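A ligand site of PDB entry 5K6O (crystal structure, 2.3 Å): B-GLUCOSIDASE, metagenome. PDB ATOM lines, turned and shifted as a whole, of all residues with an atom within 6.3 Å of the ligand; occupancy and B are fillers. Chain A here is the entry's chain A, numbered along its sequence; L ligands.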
ATOM      1  N   SER A  59      27.068 -19.356 -23.446  1.00  0.00           N
ATOM      2  CA  SER A  59      27.384 -20.327 -24.534  1.00  0.00           C
ATOM      3  C   SER A  59      26.173 -20.748 -25.364  1.00  0.00           C
ATOM      4  O   SER A  59      26.302 -20.916 -26.563  1.00  0.00           O
ATOM      5  CB  SER A  59      28.084 -21.600 -24.004  1.00  0.00           C
ATOM      6  OG  SER A  59      27.242 -22.364 -23.133  1.00  0.00           O
ATOM      7  N   GLY A  60      25.024 -20.921 -24.696  1.00  0.00           N
ATOM      8  CA  GLY A  60      23.770 -21.296 -25.348  1.00  0.00           C
ATOM      9  C   GLY A  60      22.879 -20.130 -25.763  1.00  0.00           C
ATOM     10  O   GLY A  60      21.662 -20.311 -25.882  1.00  0.00           O
ATOM     11  N   TRP A 106      31.548 -11.204 -20.824  1.00  0.00           N
ATOM     12  CA  TRP A 106      31.045 -12.592 -20.896  1.00  0.00           C
ATOM     13  C   TRP A 106      29.690 -12.798 -20.178  1.00  0.00           C
ATOM     14  O   TRP A 106      28.662 -13.076 -20.831  1.00  0.00           O
ATOM     15  CB  TRP A 106      32.115 -13.557 -20.356  1.00  0.00           C
ATOM     16  CG  TRP A 106      31.646 -14.996 -20.197  1.00  0.00           C
ATOM     17  CD1 TRP A 106      31.419 -15.671 -19.014  1.00  0.00           C
ATOM     18  CD2 TRP A 106      31.331 -15.921 -21.249  1.00  0.00           C
ATOM     19  NE1 TRP A 106      30.987 -16.956 -19.280  1.00  0.00           N
ATOM     20  CE2 TRP A 106      30.921 -17.140 -20.646  1.00  0.00           C
ATOM     21  CE3 TRP A 106      31.360 -15.841 -22.655  1.00  0.00           C
ATOM     22  CZ2 TRP A 106      30.554 -18.272 -21.395  1.00  0.00           C
ATOM     23  CZ3 TRP A 106      30.987 -16.978 -23.398  1.00  0.00           C
ATOM     24  CH2 TRP A 106      30.591 -18.168 -22.770  1.00  0.00           C
ATOM     25  N   GLU A 143      25.099 -18.141 -17.951  1.00  0.00           N
ATOM     26  CA  GLU A 143      26.305 -18.674 -17.345  1.00  0.00           C
ATOM     27  C   GLU A 143      26.941 -17.682 -16.384  1.00  0.00           C
ATOM     28  O   GLU A 143      27.036 -16.500 -16.666  1.00  0.00           O
ATOM     29  CB  GLU A 143      27.330 -19.032 -18.413  1.00  0.00           C
ATOM     30  CG  GLU A 143      27.015 -20.268 -19.212  1.00  0.00           C
ATOM     31  CD  GLU A 143      28.239 -20.806 -19.934  1.00  0.00           C
ATOM     32  OE1 GLU A 143      28.353 -20.552 -21.147  1.00  0.00           O
ATOM     33  OE2 GLU A 143      29.087 -21.462 -19.299  1.00  0.00           O
ATOM     34  N   ASP A 144      27.363 -18.206 -15.233  1.00  0.00           N
ATOM     35  CA  ASP A 144      28.202 -17.521 -14.263  1.00  0.00           C
ATOM     36  C   ASP A 144      27.564 -16.451 -13.395  1.00  0.00           C
ATOM     37  O   ASP A 144      28.031 -16.236 -12.266  1.00  0.00           O
ATOM     38  CB  ASP A 144      29.505 -17.031 -14.909  1.00  0.00           C
ATOM     39  CG  ASP A 144      30.473 -18.172 -15.164  1.00  0.00           C
ATOM     40  OD1 ASP A 144      30.844 -18.823 -14.161  1.00  0.00           O
ATOM     41  OD2 ASP A 144      30.858 -18.427 -16.325  1.00  0.00           O
ATOM     42  N   MET A 500      39.492 -23.531 -28.821  1.00  0.00           N
ATOM     43  CA  MET A 500      38.326 -23.318 -29.671  1.00  0.00           C
ATOM     44  C   MET A 500      38.752 -22.813 -31.045  1.00  0.00           C
ATOM     45  O   MET A 500      39.795 -22.134 -31.209  1.00  0.00           O
ATOM     46  CB  MET A 500      37.349 -22.326 -29.027  1.00  0.00           C
ATOM     47  CG  MET A 500      36.575 -22.893 -27.850  1.00  0.00           C
ATOM     48  SD  MET A 500      35.458 -21.686 -27.101  1.00  0.00           S
ATOM     49  CE  MET A 500      34.073 -21.796 -28.242  1.00  0.00           C
ATOM     50  N   ALA A 510      33.271 -24.972 -31.418  1.00  0.00           N
ATOM     51  CA  ALA A 510      33.853 -25.196 -30.098  1.00  0.00           C
ATOM     52  C   ALA A 510      35.028 -26.164 -30.050  1.00  0.00           C
ATOM     53  O   ALA A 510      35.917 -26.000 -29.217  1.00  0.00           O
ATOM     54  CB  ALA A 510      32.767 -25.681 -29.130  1.00  0.00           C
ATOM     55  N   ASP A 532      28.380 -25.453 -29.640  1.00  0.00           N
ATOM     56  CA  ASP A 532      27.177 -24.950 -28.949  1.00  0.00           C
ATOM     57  C   ASP A 532      26.114 -24.600 -29.976  1.00  0.00           C
ATOM     58  O   ASP A 532      26.457 -24.162 -31.065  1.00  0.00           O
ATOM     59  CB  ASP A 532      27.459 -23.656 -28.197  1.00  0.00           C
ATOM     60  CG  ASP A 532      28.259 -23.871 -26.937  1.00  0.00           C
ATOM     61  OD1 ASP A 532      27.774 -24.637 -26.065  1.00  0.00           O
ATOM     62  OD2 ASP A 532      29.354 -23.244 -26.798  1.00  0.00           O
ATOM     63  N   ARG A 538      26.055 -21.682 -32.502  1.00  0.00           N
ATOM     64  CA  ARG A 538      26.894 -20.550 -32.175  1.00  0.00           C
ATOM     65  C   ARG A 538      28.108 -20.620 -33.072  1.00  0.00           C
ATOM     66  O   ARG A 538      28.868 -21.555 -32.970  1.00  0.00           O
ATOM     67  CB  ARG A 538      27.330 -20.640 -30.714  1.00  0.00           C
ATOM     68  CG  ARG A 538      28.397 -19.659 -30.283  1.00  0.00           C
ATOM     69  CD  ARG A 538      29.034 -20.097 -28.996  1.00  0.00           C
ATOM     70  NE  ARG A 538      30.181 -19.250 -28.651  1.00  0.00           N
ATOM     71  CZ  ARG A 538      30.847 -19.309 -27.498  1.00  0.00           C
ATOM     72  NH1 ARG A 538      30.502 -20.174 -26.526  1.00  0.00           N
ATOM     73  NH2 ARG A 538      31.881 -18.490 -27.319  1.00  0.00           N
ATOM     74  N   LEU A 583      26.249 -29.261 -28.722  1.00  0.00           N
ATOM     75  CA  LEU A 583      26.444 -29.332 -27.265  1.00  0.00           C
ATOM     76  C   LEU A 583      25.118 -29.007 -26.564  1.00  0.00           C
ATOM     77  O   LEU A 583      24.897 -27.906 -26.075  1.00  0.00           O
ATOM     78  CB  LEU A 583      27.610 -28.450 -26.812  1.00  0.00           C
ATOM     79  CG  LEU A 583      28.963 -28.786 -27.460  1.00  0.00           C
ATOM     80  CD1 LEU A 583      30.053 -27.800 -27.052  1.00  0.00           C
ATOM     81  CD2 LEU A 583      29.420 -30.197 -27.148  1.00  0.00           C
ATOM     82  N   ARG A 597      21.191 -20.526 -15.329  1.00  0.00           N
ATOM     83  CA  ARG A 597      21.060 -21.309 -16.556  1.00  0.00           C
ATOM     84  C   ARG A 597      19.744 -22.068 -16.670  1.00  0.00           C
ATOM     85  O   ARG A 597      19.577 -22.844 -17.628  1.00  0.00           O
ATOM     86  CB  ARG A 597      22.218 -22.300 -16.727  1.00  0.00           C
ATOM     87  CG  ARG A 597      23.511 -21.642 -17.090  1.00  0.00           C
ATOM     88  CD  ARG A 597      24.584 -22.662 -17.396  1.00  0.00           C
ATOM     89  NE  ARG A 597      24.671 -22.991 -18.820  1.00  0.00           N
ATOM     90  CZ  ARG A 597      25.736 -23.562 -19.389  1.00  0.00           C
ATOM     91  NH1 ARG A 597      26.819 -23.868 -18.665  1.00  0.00           N
ATOM     92  NH2 ARG A 597      25.722 -23.821 -20.688  1.00  0.00           N
ATOM     93  N   GLU A 600      17.951 -22.749 -20.211  1.00  0.00           N
ATOM     94  CA  GLU A 600      18.284 -23.755 -21.227  1.00  0.00           C
ATOM     95  C   GLU A 600      18.155 -25.166 -20.718  1.00  0.00           C
ATOM     96  O   GLU A 600      18.590 -26.102 -21.381  1.00  0.00           O
ATOM     97  CB  GLU A 600      19.657 -23.491 -21.903  1.00  0.00           C
ATOM     98  CG  GLU A 600      20.931 -23.693 -21.087  1.00  0.00           C
ATOM     99  CD  GLU A 600      22.213 -23.371 -21.871  1.00  0.00           C
ATOM    100  OE1 GLU A 600      22.370 -23.828 -23.030  1.00  0.00           O
ATOM    101  OE2 GLU A 600      23.082 -22.643 -21.320  1.00  0.00           O
ATOM    102  N   LYS A 630      24.321 -32.658 -21.404  1.00  0.00           N
ATOM    103  CA  LYS A 630      25.141 -31.951 -20.395  1.00  0.00           C
ATOM    104  C   LYS A 630      24.232 -31.397 -19.308  1.00  0.00           C
ATOM    105  O   LYS A 630      23.011 -31.394 -19.511  1.00  0.00           O
ATOM    106  CB  LYS A 630      25.909 -30.804 -21.047  1.00  0.00           C
ATOM    107  CG  LYS A 630      25.057 -29.610 -21.480  1.00  0.00           C
ATOM    108  CD  LYS A 630      25.720 -28.753 -22.551  1.00  0.00           C
ATOM    109  CE  LYS A 630      25.074 -27.380 -22.623  1.00  0.00           C
ATOM    110  NZ  LYS A 630      25.700 -26.512 -23.669  1.00  0.00           N
ATOM    111  N   HIS A 631      24.765 -30.980 -18.153  1.00  0.00           N
ATOM    112  CA  HIS A 631      26.128 -31.283 -17.628  1.00  0.00           C
ATOM    113  C   HIS A 631      26.020 -32.352 -16.540  1.00  0.00           C
ATOM    114  O   HIS A 631      25.351 -32.158 -15.529  1.00  0.00           O
ATOM    115  CB  HIS A 631      26.741 -30.038 -17.036  1.00  0.00           C
ATOM    116  CG  HIS A 631      26.604 -28.834 -17.909  1.00  0.00           C
ATOM    117  ND1 HIS A 631      25.494 -28.017 -17.863  1.00  0.00           N
ATOM    118  CD2 HIS A 631      27.411 -28.319 -18.855  1.00  0.00           C
ATOM    119  CE1 HIS A 631      25.630 -27.052 -18.743  1.00  0.00           C
ATOM    120  NE2 HIS A 631      26.798 -27.207 -19.351  1.00  0.00           N
ATOM    121  N   ASN A 635      24.959 -29.935 -11.812  1.00  0.00           N
ATOM    122  CA  ASN A 635      25.294 -28.530 -12.039  1.00  0.00           C
ATOM    123  C   ASN A 635      23.980 -27.734 -11.964  1.00  0.00           C
ATOM    124  O   ASN A 635      23.388 -27.399 -12.972  1.00  0.00           O
ATOM    125  CB  ASN A 635      26.053 -28.356 -13.380  1.00  0.00           C
ATOM    126  CG  ASN A 635      26.497 -26.923 -13.643  1.00  0.00           C
ATOM    127  OD1 ASN A 635      26.979 -26.224 -12.732  1.00  0.00           O
ATOM    128  ND2 ASN A 635      26.345 -26.482 -14.876  1.00  0.00           N
ATOM    129  N   GLU A 638      25.169 -21.728 -10.703  1.00  0.00           N
ATOM    130  CA  GLU A 638      26.248 -21.075 -11.438  1.00  0.00           C
ATOM    131  C   GLU A 638      27.303 -20.438 -10.537  1.00  0.00           C
ATOM    132  O   GLU A 638      28.472 -20.483 -10.873  1.00  0.00           O
ATOM    133  CB  GLU A 638      25.682 -20.058 -12.420  1.00  0.00           C
ATOM    134  CG  GLU A 638      24.953 -20.710 -13.594  1.00  0.00           C
ATOM    135  CD  GLU A 638      25.813 -21.741 -14.331  1.00  0.00           C
ATOM    136  OE1 GLU A 638      26.772 -21.295 -15.011  1.00  0.00           O
ATOM    137  OE2 GLU A 638      25.548 -22.957 -14.210  1.00  0.00           O
ATOM    138  N   ARG A 641      30.884 -22.322  -9.663  1.00  0.00           N
ATOM    139  CA  ARG A 641      30.767 -23.622 -10.337  1.00  0.00           C
ATOM    140  C   ARG A 641      32.099 -24.258 -10.762  1.00  0.00           C
ATOM    141  O   ARG A 641      32.098 -25.391 -11.234  1.00  0.00           O
ATOM    142  CB  ARG A 641      29.848 -23.487 -11.572  1.00  0.00           C
ATOM    143  CG  ARG A 641      30.509 -22.758 -12.739  1.00  0.00           C
ATOM    144  CD  ARG A 641      29.503 -22.044 -13.604  1.00  0.00           C
ATOM    145  NE  ARG A 641      30.082 -21.580 -14.860  1.00  0.00           N
ATOM    146  CZ  ARG A 641      29.895 -22.149 -16.053  1.00  0.00           C
ATOM    147  NH1 ARG A 641      29.161 -23.247 -16.216  1.00  0.00           N
ATOM    148  NH2 ARG A 641      30.479 -21.597 -17.108  1.00  0.00           N
ATOM    149  N   MET A 674      28.601 -34.816 -21.539  1.00  0.00           N
ATOM    150  CA  MET A 674      29.560 -33.812 -21.074  1.00  0.00           C
ATOM    151  C   MET A 674      29.502 -33.730 -19.551  1.00  0.00           C
ATOM    152  O   MET A 674      28.429 -33.575 -19.004  1.00  0.00           O
ATOM    153  CB  MET A 674      29.261 -32.420 -21.663  1.00  0.00           C
ATOM    154  CG  MET A 674      30.327 -31.359 -21.329  1.00  0.00           C
ATOM    155  SD  MET A 674      29.929 -29.625 -21.677  1.00  0.00           S
ATOM    156  CE  MET A 674      29.444 -29.772 -23.394  1.00  0.00           C
ATOM    157  N   TYR A 677      31.948 -28.642 -14.418  1.00  0.00           N
ATOM    158  CA  TYR A 677      33.055 -27.857 -13.879  1.00  0.00           C
ATOM    159  C   TYR A 677      33.244 -28.055 -12.378  1.00  0.00           C
ATOM    160  O   TYR A 677      34.265 -27.645 -11.846  1.00  0.00           O
ATOM    161  CB  TYR A 677      32.780 -26.372 -14.101  1.00  0.00           C
ATOM    162  CG  TYR A 677      33.066 -25.837 -15.487  1.00  0.00           C
ATOM    163  CD1 TYR A 677      34.338 -25.912 -16.028  1.00  0.00           C
ATOM    164  CD2 TYR A 677      32.083 -25.134 -16.198  1.00  0.00           C
ATOM    165  CE1 TYR A 677      34.622 -25.371 -17.267  1.00  0.00           C
ATOM    166  CE2 TYR A 677      32.370 -24.586 -17.429  1.00  0.00           C
ATOM    167  CZ  TYR A 677      33.643 -24.708 -17.962  1.00  0.00           C
ATOM    168  OH  TYR A 677      33.934 -24.167 -19.177  1.00  0.00           O
ATOM    169  N   ASP A 709      33.738 -30.553 -19.637  1.00  0.00           N
ATOM    170  CA  ASP A 709      33.331 -29.194 -19.948  1.00  0.00           C
ATOM    171  C   ASP A 709      34.608 -28.403 -20.354  1.00  0.00           C
ATOM    172  O   ASP A 709      35.729 -28.849 -20.156  1.00  0.00           O
ATOM    173  CB  ASP A 709      32.587 -28.566 -18.755  1.00  0.00           C
ATOM    174  CG  ASP A 709      31.565 -27.497 -19.193  1.00  0.00           C
ATOM    175  OD1 ASP A 709      31.761 -26.885 -20.259  1.00  0.00           O
ATOM    176  OD2 ASP A 709      30.566 -27.273 -18.463  1.00  0.00           O
ATOM    177  N   TRP A 710      34.426 -27.237 -20.959  1.00  0.00           N
ATOM    178  CA  TRP A 710      35.536 -26.550 -21.626  1.00  0.00           C
ATOM    179  C   TRP A 710      36.558 -25.913 -20.654  1.00  0.00           C
ATOM    180  O   TRP A 710      36.253 -24.915 -19.968  1.00  0.00           O
ATOM    181  CB  TRP A 710      34.983 -25.493 -22.590  1.00  0.00           C
ATOM    182  CG  TRP A 710      34.931 -25.954 -24.009  1.00  0.00           C
ATOM    183  CD1 TRP A 710      35.510 -25.322 -25.060  1.00  0.00           C
ATOM    184  CD2 TRP A 710      34.292 -27.118 -24.528  1.00  0.00           C
ATOM    185  NE1 TRP A 710      35.267 -26.018 -26.209  1.00  0.00           N
ATOM    186  CE2 TRP A 710      34.513 -27.119 -25.922  1.00  0.00           C
ATOM    187  CE3 TRP A 710      33.525 -28.143 -23.965  1.00  0.00           C
ATOM    188  CZ2 TRP A 710      34.010 -28.123 -26.755  1.00  0.00           C
ATOM    189  CZ3 TRP A 710      33.026 -29.147 -24.811  1.00  0.00           C
ATOM    190  CH2 TRP A 710      33.282 -29.126 -26.181  1.00  0.00           C
ATOM    191  N   TRP A 711      37.762 -26.465 -20.652  1.00  0.00           N
ATOM    192  CA  TRP A 711      38.842 -26.077 -19.727  1.00  0.00           C
ATOM    193  C   TRP A 711      38.503 -26.398 -18.270  1.00  0.00           C
ATOM    194  O   TRP A 711      38.927 -25.681 -17.333  1.00  0.00           O
ATOM    195  CB  TRP A 711      39.248 -24.597 -19.875  1.00  0.00           C
ATOM    196  CG  TRP A 711      39.669 -24.248 -21.235  1.00  0.00           C
ATOM    197  CD1 TRP A 711      40.798 -24.657 -21.875  1.00  0.00           C
ATOM    198  CD2 TRP A 711      38.959 -23.397 -22.148  1.00  0.00           C
ATOM    199  NE1 TRP A 711      40.835 -24.131 -23.142  1.00  0.00           N
ATOM    200  CE2 TRP A 711      39.718 -23.350 -23.334  1.00  0.00           C
ATOM    201  CE3 TRP A 711      37.754 -22.677 -22.070  1.00  0.00           C
ATOM    202  CZ2 TRP A 711      39.322 -22.589 -24.449  1.00  0.00           C
ATOM    203  CZ3 TRP A 711      37.352 -21.922 -23.179  1.00  0.00           C
ATOM    204  CH2 TRP A 711      38.134 -21.892 -24.358  1.00  0.00           C
HETATM  205  C1  LIG L   1      31.235 -23.877 -21.331  1.00  0.00           C
HETATM  206  C2  LIG L   1      29.797 -24.286 -20.886  1.00  0.00           C
HETATM  207  C3  LIG L   1      29.309 -25.550 -21.647  1.00  0.00           C
HETATM  208  C4  LIG L   1      29.980 -25.889 -23.033  1.00  0.00           C
HETATM  209  C5  LIG L   1      31.235 -25.040 -23.438  1.00  0.00           C
HETATM  210  C6  LIG L   1      31.438 -24.782 -24.942  1.00  0.00           C
HETATM  211  O1  LIG L   1      31.686 -22.609 -20.868  1.00  0.00           O
HETATM  212  O2  LIG L   1      29.608 -24.481 -19.445  1.00  0.00           O
HETATM  213  O3  LIG L   1      27.874 -25.499 -21.743  1.00  0.00           O
HETATM  214  O4  LIG L   1      28.985 -25.932 -24.068  1.00  0.00           O
HETATM  215  O5  LIG L   1      31.274 -23.773 -22.756  1.00  0.00           O
HETATM  216  O6  LIG L   1      31.607 -23.393 -25.255  1.00  0.00           O
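The guanidinium group (NH2) of Arg 641 lies within salt-bridge range of the side-chain carboxylate (OE2) of Glu 143, at 2.6 Å.
NH2 of Arg 597 lies within salt-bridge range of OE2 of Glu 600 (3.0 Å).
The side-chain carboxylate of Asp 532 lies within salt-bridge range of the side-chain amino group of Lys 630, 3.7 Å away.
The guanidinium group (NH1) of Arg 597 lies within salt-bridge range of the side-chain carboxylate (OE2) of Glu 143.
OE1 of Glu 638 lies within salt-bridge range of NH1 of Arg 641, 3.3 Å away.
The side-chain hydroxyl (OH) of Tyr 677 is in hydrogen-bond range of the backbone carbonyl oxygen (O) of Trp 710, 2.6 Å away.
NZ of Lys 630 sits at hydrogen-bond distance from O of Leu 583 (2.9 Å).
The guanidinium group of Arg 641 lies within salt-bridge range of the side-chain carboxylate of Asp 144.
Arg 538 touches the ligand (NH1 to O6, 3.6 Å).
CD1 of Leu 583 touches O4 of the ligand (3.7 Å).
Met 674 touches the ligand (CE to O4, 3.9 Å).
Trp 710 touches the ligand.
Hydrophobic or aromatic side chains within 4 Å of the ligand: Leu 583, Met 674, Tyr 677 and Trp 710.
Within 4 Å of the ligand: Ser 59, Glu 143, Asp 532, Arg 538, Leu 583, Arg 597, Lys 630, His 631, Arg 641, Met 674, Tyr 677, Asp 709 and Trp 710.
The nearest printed residue that does not touch the ligand is Met 500 (4.2 Å).
The side-chain carboxylate (OD2) of Asp 709 lies within hydrogen-bond range of an oxygen (O2) of the ligand, at 3.1 Å.
The side-chain hydroxyl (OG) of Ser 59 is in hydrogen-bond range of an oxygen (O3) of the ligand (3.5 Å).
NH2 of Arg 597 is in hydrogen-bond range of O3 of the ligand, at 2.9 Å.
The side-chain carboxylate (OE2) of Glu 143 lies within hydrogen-bond range of an oxygen (O2) of the ligand (3.1 Å).
OH of Tyr 677 sits at hydrogen-bond distance from O1 of the ligand, 3.2 Å away.
NE2 of His 631 lies within hydrogen-bond range of O3 of the ligand (3.1 Å).
The guanidinium group (NH1) of Arg 641 is in hydrogen-bond range of an oxygen (O2) of the ligand, 3.5 Å away.
An oxygen (O4) of the ligand sits at hydrogen-bond distance from the side-chain carboxylate (OD1) of Asp 532.
The side-chain amino group (NZ) of Lys 630 is in hydrogen-bond range of an oxygen (O3) of the ligand (3.1 Å).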
